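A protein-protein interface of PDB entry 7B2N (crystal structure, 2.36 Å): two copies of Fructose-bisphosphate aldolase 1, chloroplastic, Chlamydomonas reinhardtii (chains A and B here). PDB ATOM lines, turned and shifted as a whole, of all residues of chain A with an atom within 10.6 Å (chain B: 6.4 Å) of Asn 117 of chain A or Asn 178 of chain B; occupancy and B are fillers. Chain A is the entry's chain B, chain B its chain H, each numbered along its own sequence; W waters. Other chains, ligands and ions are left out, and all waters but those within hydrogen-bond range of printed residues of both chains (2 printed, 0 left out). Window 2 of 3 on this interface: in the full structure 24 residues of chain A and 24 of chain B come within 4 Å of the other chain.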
ATOM      1  N   VAL A 113      29.539  19.081  14.627  1.00  0.00           N
ATOM      2  CA  VAL A 113      29.855  18.296  13.434  1.00  0.00           C
ATOM      3  C   VAL A 113      30.395  19.268  12.392  1.00  0.00           C
ATOM      4  O   VAL A 113      29.939  20.420  12.346  1.00  0.00           O
ATOM      5  CB  VAL A 113      28.614  17.549  12.906  1.00  0.00           C
ATOM      6  CG1 VAL A 113      28.988  16.569  11.804  1.00  0.00           C
ATOM      7  CG2 VAL A 113      27.883  16.817  14.030  1.00  0.00           C
ATOM      8  N   PRO A 114      31.360  18.881  11.556  1.00  0.00           N
ATOM      9  CA  PRO A 114      31.808  19.787  10.490  1.00  0.00           C
ATOM     10  C   PRO A 114      30.663  20.188   9.571  1.00  0.00           C
ATOM     11  O   PRO A 114      29.904  19.349   9.082  1.00  0.00           O
ATOM     12  CB  PRO A 114      32.877  18.975   9.744  1.00  0.00           C
ATOM     13  CG  PRO A 114      32.857  17.590  10.358  1.00  0.00           C
ATOM     14  CD  PRO A 114      32.276  17.740  11.720  1.00  0.00           C
ATOM     15  N   LEU A 115      30.539  21.493   9.357  1.00  0.00           N
ATOM     16  CA  LEU A 115      29.566  22.034   8.422  1.00  0.00           C
ATOM     17  C   LEU A 115      30.130  21.980   7.008  1.00  0.00           C
ATOM     18  O   LEU A 115      31.237  22.469   6.753  1.00  0.00           O
ATOM     19  CB  LEU A 115      29.216  23.469   8.810  1.00  0.00           C
ATOM     20  CG  LEU A 115      28.177  24.195   7.969  1.00  0.00           C
ATOM     21  CD1 LEU A 115      26.911  23.369   7.851  1.00  0.00           C
ATOM     22  CD2 LEU A 115      27.884  25.540   8.600  1.00  0.00           C
ATOM     23  N   SER A 116      29.368  21.381   6.096  1.00  0.00           N
ATOM     24  CA  SER A 116      29.850  21.145   4.741  1.00  0.00           C
ATOM     25  C   SER A 116      30.129  22.456   4.014  1.00  0.00           C
ATOM     26  O   SER A 116      29.374  23.426   4.129  1.00  0.00           O
ATOM     27  CB  SER A 116      28.835  20.311   3.958  1.00  0.00           C
ATOM     28  OG  SER A 116      28.556  19.087   4.617  1.00  0.00           O
ATOM     29  N   ASN A 117      31.238  22.476   3.271  1.00  0.00           N
ATOM     30  CA  ASN A 117      31.654  23.588   2.417  1.00  0.00           C
ATOM     31  C   ASN A 117      32.080  24.822   3.202  1.00  0.00           C
ATOM     32  O   ASN A 117      32.096  25.928   2.658  1.00  0.00           O
ATOM     33  CB  ASN A 117      30.564  23.957   1.402  1.00  0.00           C
ATOM     34  CG  ASN A 117      30.290  22.837   0.419  1.00  0.00           C
ATOM     35  OD1 ASN A 117      31.070  21.887   0.318  1.00  0.00           O
ATOM     36  ND2 ASN A 117      29.186  22.943  -0.316  1.00  0.00           N
ATOM     37  N   THR A 118      32.429  24.662   4.471  1.00  0.00           N
ATOM     38  CA  THR A 118      33.127  25.690   5.223  1.00  0.00           C
ATOM     39  C   THR A 118      34.575  25.262   5.408  1.00  0.00           C
ATOM     40  O   THR A 118      34.917  24.083   5.285  1.00  0.00           O
ATOM     41  CB  THR A 118      32.474  25.937   6.594  1.00  0.00           C
ATOM     42  OG1 THR A 118      32.648  24.786   7.432  1.00  0.00           O
ATOM     43  CG2 THR A 118      30.992  26.233   6.444  1.00  0.00           C
ATOM     44  N   ASN A 119      35.434  26.236   5.707  1.00  0.00           N
ATOM     45  CA  ASN A 119      36.831  25.937   6.014  1.00  0.00           C
ATOM     46  C   ASN A 119      36.937  25.649   7.510  1.00  0.00           C
ATOM     47  O   ASN A 119      37.308  26.501   8.319  1.00  0.00           O
ATOM     48  CB  ASN A 119      37.743  27.081   5.589  1.00  0.00           C
ATOM     49  CG  ASN A 119      39.213  26.733   5.730  1.00  0.00           C
ATOM     50  OD1 ASN A 119      39.620  25.599   5.468  1.00  0.00           O
ATOM     51  ND2 ASN A 119      40.015  27.703   6.158  1.00  0.00           N
ATOM     52  N   GLY A 120      36.572  24.421   7.876  1.00  0.00           N
ATOM     53  CA  GLY A 120      36.765  23.948   9.234  1.00  0.00           C
ATOM     54  C   GLY A 120      35.781  24.449  10.270  1.00  0.00           C
ATOM     55  O   GLY A 120      36.140  24.564  11.447  1.00  0.00           O
ATOM     56  N   GLU A 121      34.543  24.735   9.882  1.00  0.00           N
ATOM     57  CA  GLU A 121      33.557  25.235  10.828  1.00  0.00           C
ATOM     58  C   GLU A 121      32.571  24.144  11.228  1.00  0.00           C
ATOM     59  O   GLU A 121      32.334  23.189  10.486  1.00  0.00           O
ATOM     60  CB  GLU A 121      32.802  26.427  10.247  1.00  0.00           C
ATOM     61  CG  GLU A 121      33.546  27.734  10.419  1.00  0.00           C
ATOM     62  CD  GLU A 121      32.883  28.872   9.690  1.00  0.00           C
ATOM     63  OE1 GLU A 121      32.637  28.723   8.474  1.00  0.00           O
ATOM     64  OE2 GLU A 121      32.601  29.909  10.328  1.00  0.00           O
ATOM     65  N   SER A 122      31.988  24.311  12.411  1.00  0.00           N
ATOM     66  CA  SER A 122      31.080  23.340  12.994  1.00  0.00           C
ATOM     67  C   SER A 122      29.643  23.839  12.950  1.00  0.00           C
ATOM     68  O   SER A 122      29.374  25.043  12.864  1.00  0.00           O
ATOM     69  CB  SER A 122      31.468  23.034  14.444  1.00  0.00           C
ATOM     70  OG  SER A 122      32.782  22.512  14.521  1.00  0.00           O
ATOM     71  N   TRP A 123      28.721  22.878  12.990  1.00  0.00           N
ATOM     72  CA  TRP A 123      27.324  23.116  13.310  1.00  0.00           C
ATOM     73  C   TRP A 123      26.911  22.115  14.380  1.00  0.00           C
ATOM     74  O   TRP A 123      27.585  21.105  14.614  1.00  0.00           O
ATOM     75  CB  TRP A 123      26.408  22.999  12.080  1.00  0.00           C
ATOM     76  CG  TRP A 123      26.305  21.612  11.499  1.00  0.00           C
ATOM     77  CD1 TRP A 123      27.275  20.934  10.815  1.00  0.00           C
ATOM     78  CD2 TRP A 123      25.161  20.743  11.536  1.00  0.00           C
ATOM     79  NE1 TRP A 123      26.809  19.699  10.430  1.00  0.00           N
ATOM     80  CE2 TRP A 123      25.516  19.556  10.863  1.00  0.00           C
ATOM     81  CE3 TRP A 123      23.875  20.853  12.076  1.00  0.00           C
ATOM     82  CZ2 TRP A 123      24.630  18.488  10.714  1.00  0.00           C
ATOM     83  CZ3 TRP A 123      22.995  19.790  11.924  1.00  0.00           C
ATOM     84  CH2 TRP A 123      23.378  18.625  11.250  1.00  0.00           C
ATOM     85  N   HIS A 155      37.519  31.918  11.750  1.00  0.00           N
ATOM     86  CA  HIS A 155      36.923  31.548  10.473  1.00  0.00           C
ATOM     87  C   HIS A 155      35.937  32.589   9.954  1.00  0.00           C
ATOM     88  O   HIS A 155      35.338  32.382   8.894  1.00  0.00           O
ATOM     89  CB  HIS A 155      36.232  30.189  10.591  1.00  0.00           C
ATOM     90  CG  HIS A 155      37.166  29.062  10.900  1.00  0.00           C
ATOM     91  ND1 HIS A 155      37.102  28.344  12.076  1.00  0.00           N
ATOM     92  CD2 HIS A 155      38.189  28.530  10.189  1.00  0.00           C
ATOM     93  CE1 HIS A 155      38.042  27.414  12.073  1.00  0.00           C
ATOM     94  NE2 HIS A 155      38.715  27.508  10.940  1.00  0.00           N
ATOM     95  N   PRO A 157      32.916  34.530  11.758  1.00  0.00           N
ATOM     96  CA  PRO A 157      32.449  33.283  11.135  1.00  0.00           C
ATOM     97  C   PRO A 157      31.858  33.466   9.737  1.00  0.00           C
ATOM     98  O   PRO A 157      31.489  34.580   9.369  1.00  0.00           O
ATOM     99  CB  PRO A 157      31.370  32.800  12.107  1.00  0.00           C
ATOM    100  CG  PRO A 157      30.825  34.052  12.682  1.00  0.00           C
ATOM    101  CD  PRO A 157      32.012  34.969  12.835  1.00  0.00           C
ATOM    102  N   SER A 158      31.777  32.379   8.972  1.00  0.00           N
ATOM    103  CA  SER A 158      31.152  32.448   7.662  1.00  0.00           C
ATOM    104  C   SER A 158      29.660  32.731   7.806  1.00  0.00           C
ATOM    105  O   SER A 158      29.063  32.560   8.875  1.00  0.00           O
ATOM    106  CB  SER A 158      31.356  31.147   6.887  1.00  0.00           C
ATOM    107  OG  SER A 158      30.485  30.133   7.343  1.00  0.00           O
ATOM    108  N   ILE A 159      29.057  33.177   6.705  1.00  0.00           N
ATOM    109  CA  ILE A 159      27.634  33.507   6.725  1.00  0.00           C
ATOM    110  C   ILE A 159      26.805  32.266   7.036  1.00  0.00           C
ATOM    111  O   ILE A 159      25.897  32.301   7.874  1.00  0.00           O
ATOM    112  CB  ILE A 159      27.213  34.153   5.392  1.00  0.00           C
ATOM    113  CG1 ILE A 159      27.812  35.555   5.272  1.00  0.00           C
ATOM    114  CG2 ILE A 159      25.699  34.221   5.284  1.00  0.00           C
ATOM    115  CD1 ILE A 159      27.410  36.279   3.997  1.00  0.00           C
ATOM    116  N   ILE A 160      27.111  31.146   6.377  1.00  0.00           N
ATOM    117  CA  ILE A 160      26.285  29.955   6.565  1.00  0.00           C
ATOM    118  C   ILE A 160      26.556  29.299   7.914  1.00  0.00           C
ATOM    119  O   ILE A 160      25.662  28.665   8.488  1.00  0.00           O
ATOM    120  CB  ILE A 160      26.485  28.964   5.404  1.00  0.00           C
ATOM    121  CG1 ILE A 160      27.934  28.478   5.346  1.00  0.00           C
ATOM    122  CG2 ILE A 160      26.066  29.603   4.085  1.00  0.00           C
ATOM    123  CD1 ILE A 160      28.153  27.376   4.336  1.00  0.00           C
ATOM    124  N   ALA A 161      27.769  29.431   8.449  1.00  0.00           N
ATOM    125  CA  ALA A 161      28.030  28.908   9.788  1.00  0.00           C
ATOM    126  C   ALA A 161      27.267  29.697  10.840  1.00  0.00           C
ATOM    127  O   ALA A 161      26.662  29.118  11.751  1.00  0.00           O
ATOM    128  CB  ALA A 161      29.528  28.921  10.088  1.00  0.00           C
ATOM    129  N   LYS B  11      36.991  16.480  -5.114  1.00  0.00           N
ATOM    130  CA  LYS B  11      37.306  15.068  -4.905  1.00  0.00           C
ATOM    131  C   LYS B  11      36.259  14.162  -5.536  1.00  0.00           C
ATOM    132  O   LYS B  11      36.587  13.190  -6.213  1.00  0.00           O
ATOM    133  CB  LYS B  11      37.426  14.760  -3.417  1.00  0.00           C
ATOM    134  CG  LYS B  11      37.858  13.336  -3.124  1.00  0.00           C
ATOM    135  CD  LYS B  11      36.794  12.594  -2.340  1.00  0.00           C
ATOM    136  CE  LYS B  11      37.379  11.397  -1.613  1.00  0.00           C
ATOM    137  NZ  LYS B  11      38.392  11.795  -0.595  1.00  0.00           N
ATOM    138  N   TYR B  12      34.990  14.478  -5.292  1.00  0.00           N
ATOM    139  CA  TYR B  12      33.878  13.832  -5.971  1.00  0.00           C
ATOM    140  C   TYR B  12      33.316  14.691  -7.092  1.00  0.00           C
ATOM    141  O   TYR B  12      32.339  14.291  -7.737  1.00  0.00           O
ATOM    142  CB  TYR B  12      32.768  13.493  -4.969  1.00  0.00           C
ATOM    143  CG  TYR B  12      33.164  12.447  -3.949  1.00  0.00           C
ATOM    144  CD1 TYR B  12      33.553  11.173  -4.348  1.00  0.00           C
ATOM    145  CD2 TYR B  12      33.145  12.731  -2.588  1.00  0.00           C
ATOM    146  CE1 TYR B  12      33.916  10.213  -3.423  1.00  0.00           C
ATOM    147  CE2 TYR B  12      33.502  11.775  -1.652  1.00  0.00           C
ATOM    148  CZ  TYR B  12      33.889  10.520  -2.076  1.00  0.00           C
ATOM    149  OH  TYR B  12      34.250   9.566  -1.154  1.00  0.00           O
ATOM    150  N   LEU B  16      30.564  13.333  -9.619  1.00  0.00           N
ATOM    151  CA  LEU B  16      29.208  13.849  -9.468  1.00  0.00           C
ATOM    152  C   LEU B  16      28.665  14.336 -10.804  1.00  0.00           C
ATOM    153  O   LEU B  16      27.486  14.128 -11.119  1.00  0.00           O
ATOM    154  CB  LEU B  16      29.177  14.972  -8.428  1.00  0.00           C
ATOM    155  CG  LEU B  16      29.320  14.562  -6.957  1.00  0.00           C
ATOM    156  CD1 LEU B  16      29.627  15.769  -6.088  1.00  0.00           C
ATOM    157  CD2 LEU B  16      28.081  13.844  -6.453  1.00  0.00           C
ATOM    158  N   ALA B 173      21.683  18.869   0.248  1.00  0.00           N
ATOM    159  CA  ALA B 173      22.404  18.866  -1.022  1.00  0.00           C
ATOM    160  C   ALA B 173      23.904  19.034  -0.810  1.00  0.00           C
ATOM    161  O   ALA B 173      24.708  18.330  -1.433  1.00  0.00           O
ATOM    162  CB  ALA B 173      21.861  19.963  -1.938  1.00  0.00           C
ATOM    163  N   ALA B 174      24.301  19.941   0.087  1.00  0.00           N
ATOM    164  CA  ALA B 174      25.723  20.133   0.364  1.00  0.00           C
ATOM    165  C   ALA B 174      26.331  18.908   1.036  1.00  0.00           C
ATOM    166  O   ALA B 174      27.480  18.545   0.751  1.00  0.00           O
ATOM    167  CB  ALA B 174      25.925  21.375   1.229  1.00  0.00           C
ATOM    168  N   ILE B 175      25.582  18.262   1.935  1.00  0.00           N
ATOM    169  CA  ILE B 175      26.098  17.081   2.623  1.00  0.00           C
ATOM    170  C   ILE B 175      26.258  15.923   1.647  1.00  0.00           C
ATOM    171  O   ILE B 175      27.284  15.233   1.639  1.00  0.00           O
ATOM    172  CB  ILE B 175      25.181  16.698   3.800  1.00  0.00           C
ATOM    173  CG1 ILE B 175      25.252  17.748   4.911  1.00  0.00           C
ATOM    174  CG2 ILE B 175      25.547  15.323   4.333  1.00  0.00           C
ATOM    175  CD1 ILE B 175      24.087  17.683   5.884  1.00  0.00           C
ATOM    176  N   ALA B 176      25.241  15.692   0.811  1.00  0.00           N
ATOM    177  CA  ALA B 176      25.280  14.570  -0.122  1.00  0.00           C
ATOM    178  C   ALA B 176      26.428  14.708  -1.119  1.00  0.00           C
ATOM    179  O   ALA B 176      27.116  13.725  -1.422  1.00  0.00           O
ATOM    180  CB  ALA B 176      23.942  14.450  -0.852  1.00  0.00           C
ATOM    181  N   GLN B 177      26.655  15.920  -1.635  1.00  0.00           N
ATOM    182  CA  GLN B 177      27.746  16.123  -2.588  1.00  0.00           C
ATOM    183  C   GLN B 177      29.099  15.838  -1.948  1.00  0.00           C
ATOM    184  O   GLN B 177      29.956  15.183  -2.553  1.00  0.00           O
ATOM    185  CB  GLN B 177      27.714  17.547  -3.143  1.00  0.00           C
ATOM    186  CG  GLN B 177      26.493  17.860  -3.985  1.00  0.00           C
ATOM    187  CD  GLN B 177      26.719  19.017  -4.938  1.00  0.00           C
ATOM    188  OE1 GLN B 177      27.394  19.996  -4.602  1.00  0.00           O
ATOM    189  NE2 GLN B 177      26.158  18.908  -6.139  1.00  0.00           N
ATOM    190  N   ASN B 178      29.307  16.313  -0.719  1.00  0.00           N
ATOM    191  CA  ASN B 178      30.567  16.059  -0.030  1.00  0.00           C
ATOM    192  C   ASN B 178      30.748  14.592   0.333  1.00  0.00           C
ATOM    193  O   ASN B 178      31.869  14.181   0.653  1.00  0.00           O
ATOM    194  CB  ASN B 178      30.658  16.916   1.230  1.00  0.00           C
ATOM    195  CG  ASN B 178      31.205  18.297   0.948  1.00  0.00           C
ATOM    196  OD1 ASN B 178      32.416  18.495   0.902  1.00  0.00           O
ATOM    197  ND2 ASN B 178      30.312  19.263   0.758  1.00  0.00           N
ATOM    198  N   ALA B 179      29.681  13.796   0.299  1.00  0.00           N
ATOM    199  CA  ALA B 179      29.794  12.358   0.505  1.00  0.00           C
ATOM    200  C   ALA B 179      29.899  11.580  -0.801  1.00  0.00           C
ATOM    201  O   ALA B 179      30.137  10.369  -0.767  1.00  0.00           O
ATOM    202  CB  ALA B 179      28.598  11.841   1.316  1.00  0.00           C
ATOM    203  N   GLY B 180      29.727  12.240  -1.943  1.00  0.00           N
ATOM    204  CA  GLY B 180      29.868  11.600  -3.231  1.00  0.00           C
ATOM    205  C   GLY B 180      28.578  11.201  -3.905  1.00  0.00           C
ATOM    206  O   GLY B 180      28.621  10.431  -4.869  1.00  0.00           O
ATOM    207  N   LEU B 181      27.437  11.693  -3.434  1.00  0.00           N
ATOM    208  CA  LEU B 181      26.142  11.357  -4.008  1.00  0.00           C
ATOM    209  C   LEU B 181      25.529  12.595  -4.644  1.00  0.00           C
ATOM    210  O   LEU B 181      25.534  13.675  -4.043  1.00  0.00           O
ATOM    211  CB  LEU B 181      25.197  10.797  -2.946  1.00  0.00           C
ATOM    212  CG  LEU B 181      25.679   9.642  -2.068  1.00  0.00           C
ATOM    213  CD1 LEU B 181      24.624   9.363  -1.020  1.00  0.00           C
ATOM    214  CD2 LEU B 181      25.934   8.406  -2.887  1.00  0.00           C
ATOM    215  N   ASN B 218      25.222  27.809   0.174  1.00  0.00           N
ATOM    216  CA  ASN B 218      25.915  26.620   0.651  1.00  0.00           C
ATOM    217  C   ASN B 218      26.973  26.115  -0.322  1.00  0.00           C
ATOM    218  O   ASN B 218      27.566  25.058  -0.068  1.00  0.00           O
ATOM    219  CB  ASN B 218      24.907  25.507   0.943  1.00  0.00           C
ATOM    220  CG  ASN B 218      24.003  25.833   2.111  1.00  0.00           C
ATOM    221  OD1 ASN B 218      24.210  26.817   2.820  1.00  0.00           O
ATOM    222  ND2 ASN B 218      22.990  25.003   2.319  1.00  0.00           N
ATOM    223  N   LYS B 219      27.215  26.835  -1.420  1.00  0.00           N
ATOM    224  CA  LYS B 219      28.232  26.473  -2.410  1.00  0.00           C
ATOM    225  C   LYS B 219      27.972  25.099  -3.024  1.00  0.00           C
ATOM    226  O   LYS B 219      28.908  24.374  -3.368  1.00  0.00           O
ATOM    227  CB  LYS B 219      29.637  26.543  -1.807  1.00  0.00           C
ATOM    228  CG  LYS B 219      30.005  27.938  -1.334  1.00  0.00           C
ATOM    229  CD  LYS B 219      31.238  27.942  -0.446  1.00  0.00           C
ATOM    230  CE  LYS B 219      31.783  29.361  -0.286  1.00  0.00           C
ATOM    231  NZ  LYS B 219      30.701  30.368  -0.050  1.00  0.00           N
ATOM    232  N   VAL B 220      26.699  24.731  -3.166  1.00  0.00           N
ATOM    233  CA  VAL B 220      26.345  23.489  -3.840  1.00  0.00           C
ATOM    234  C   VAL B 220      26.671  23.611  -5.323  1.00  0.00           C
ATOM    235  O   VAL B 220      26.340  24.616  -5.964  1.00  0.00           O
ATOM    236  CB  VAL B 220      24.860  23.166  -3.627  1.00  0.00           C
ATOM    237  CG1 VAL B 220      24.459  21.968  -4.467  1.00  0.00           C
ATOM    238  CG2 VAL B 220      24.575  22.919  -2.149  1.00  0.00           C
ATOM    239  N   MET B 221      27.314  22.583  -5.876  1.00  0.00           N
ATOM    240  CA  MET B 221      27.685  22.580  -7.289  1.00  0.00           C
ATOM    241  C   MET B 221      26.467  22.215  -8.127  1.00  0.00           C
ATOM    242  O   MET B 221      26.033  21.058  -8.136  1.00  0.00           O
ATOM    243  CB  MET B 221      28.828  21.607  -7.547  1.00  0.00           C
ATOM    244  CG  MET B 221      29.328  21.642  -8.985  1.00  0.00           C
ATOM    245  SD  MET B 221      30.145  20.118  -9.480  1.00  0.00           S
ATOM    246  CE  MET B 221      31.631  20.239  -8.508  1.00  0.00           C
HETATM  247  O   HOH W   1      29.438  20.593  -2.549  1.00  0.00           O
HETATM  248  O   HOH W   2      33.289  20.429   3.146  1.00  0.00           O
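ND2 of Asn 178 of chain B lies within hydrogen-bond range of O of Ala 174 of chain B, at 2.9 Å.
Hydrophobic or aromatic side chains of chain B that line the printed part of chain A: Ala 174 and Ile 175.
Of the 17 printed residues of chain A, 3 touch a printed residue of chain B.
Among the printed residues, 8 pairs touch across the chains.
Water W2 lies within hydrogen-bond range of N of Asn 117 of chain A (2.9 Å) and OD1 of Asn 178 of chain B (3.1 Å).
Water W1 bridges the side-chain amide oxygen of Gln 177 of chain B (3.0 Å) and the side-chain amide nitrogen of Asn 117 of chain A (3.3 Å).
Asn 117 of chain A touches just these residues of chain B: Ala 174, Asn 178, Asn 218 and Lys 219.
Of the printed residues of chain A, Asn 178 of chain B touches Ser 116 and Asn 117.
No residue of chain A comes within 4 Å of Ala 176 of chain B.
Ala 179 of chain B touches none of the printed residues of chain A.
Of the printed residues of chain A, Lys 219 of chain B touches Asn 117 (3.4 Å).
Val 220 of chain B touches none of the printed residues of chain A.
Printed residues of chain B within 4 Å of Ser 116 of chain A: Ala 174, Ile 175 and Asn 178.
Of the printed residues of chain B, Ile 160 of chain A touches Asn 218 (3.6 Å).
Of the printed residues of chain A, Ile 175 of chain B touches Ser 116.
Of the printed residues of chain A, Asn 218 of chain B touches Asn 117 and Ile 160.
Leu 16 of chain B touches none of the printed residues of chain A.
The nearest residue of chain B that does not touch Asn 117 of chain A is Val 220 of chain B (4.2 Å).
The nearest residue of chain A that does not touch Asn 178 of chain B is Leu 115 of chain A (6.8 Å).
The backbone carbonyl oxygen of Asn 218 of chain B lies within hydrogen-bond range of the side-chain amide nitrogen of Asn 117 of chain A, at 2.7 Å.
The backbone carbonyl oxygen of Lys 219 of chain B lies within hydrogen-bond range of the side-chain amide nitrogen of Asn 117 of chain A (3.4 Å).
The side-chain amide nitrogen (ND2) of Asn 178 of chain B is in hydrogen-bond range of the side-chain amide oxygen (OD1) of Asn 117 of chain A.
No position is printed for both chains.
Ser 116 of chain A touches Ala 174 of chain B (CB to O, 3.9 Å).
Ile 175 of chain B touches Ser 116 of chain A.
CB of Ser 116 of chain A touches ND2 of Asn 178 of chain B, at 3.7 Å.
ND2 of Asn 117 of chain A touches CB of Ala 174 of chain B, 3.9 Å away.
OD1 of Asn 218 of chain B touches CG2 of Ile 160 of chain A (3.6 Å).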
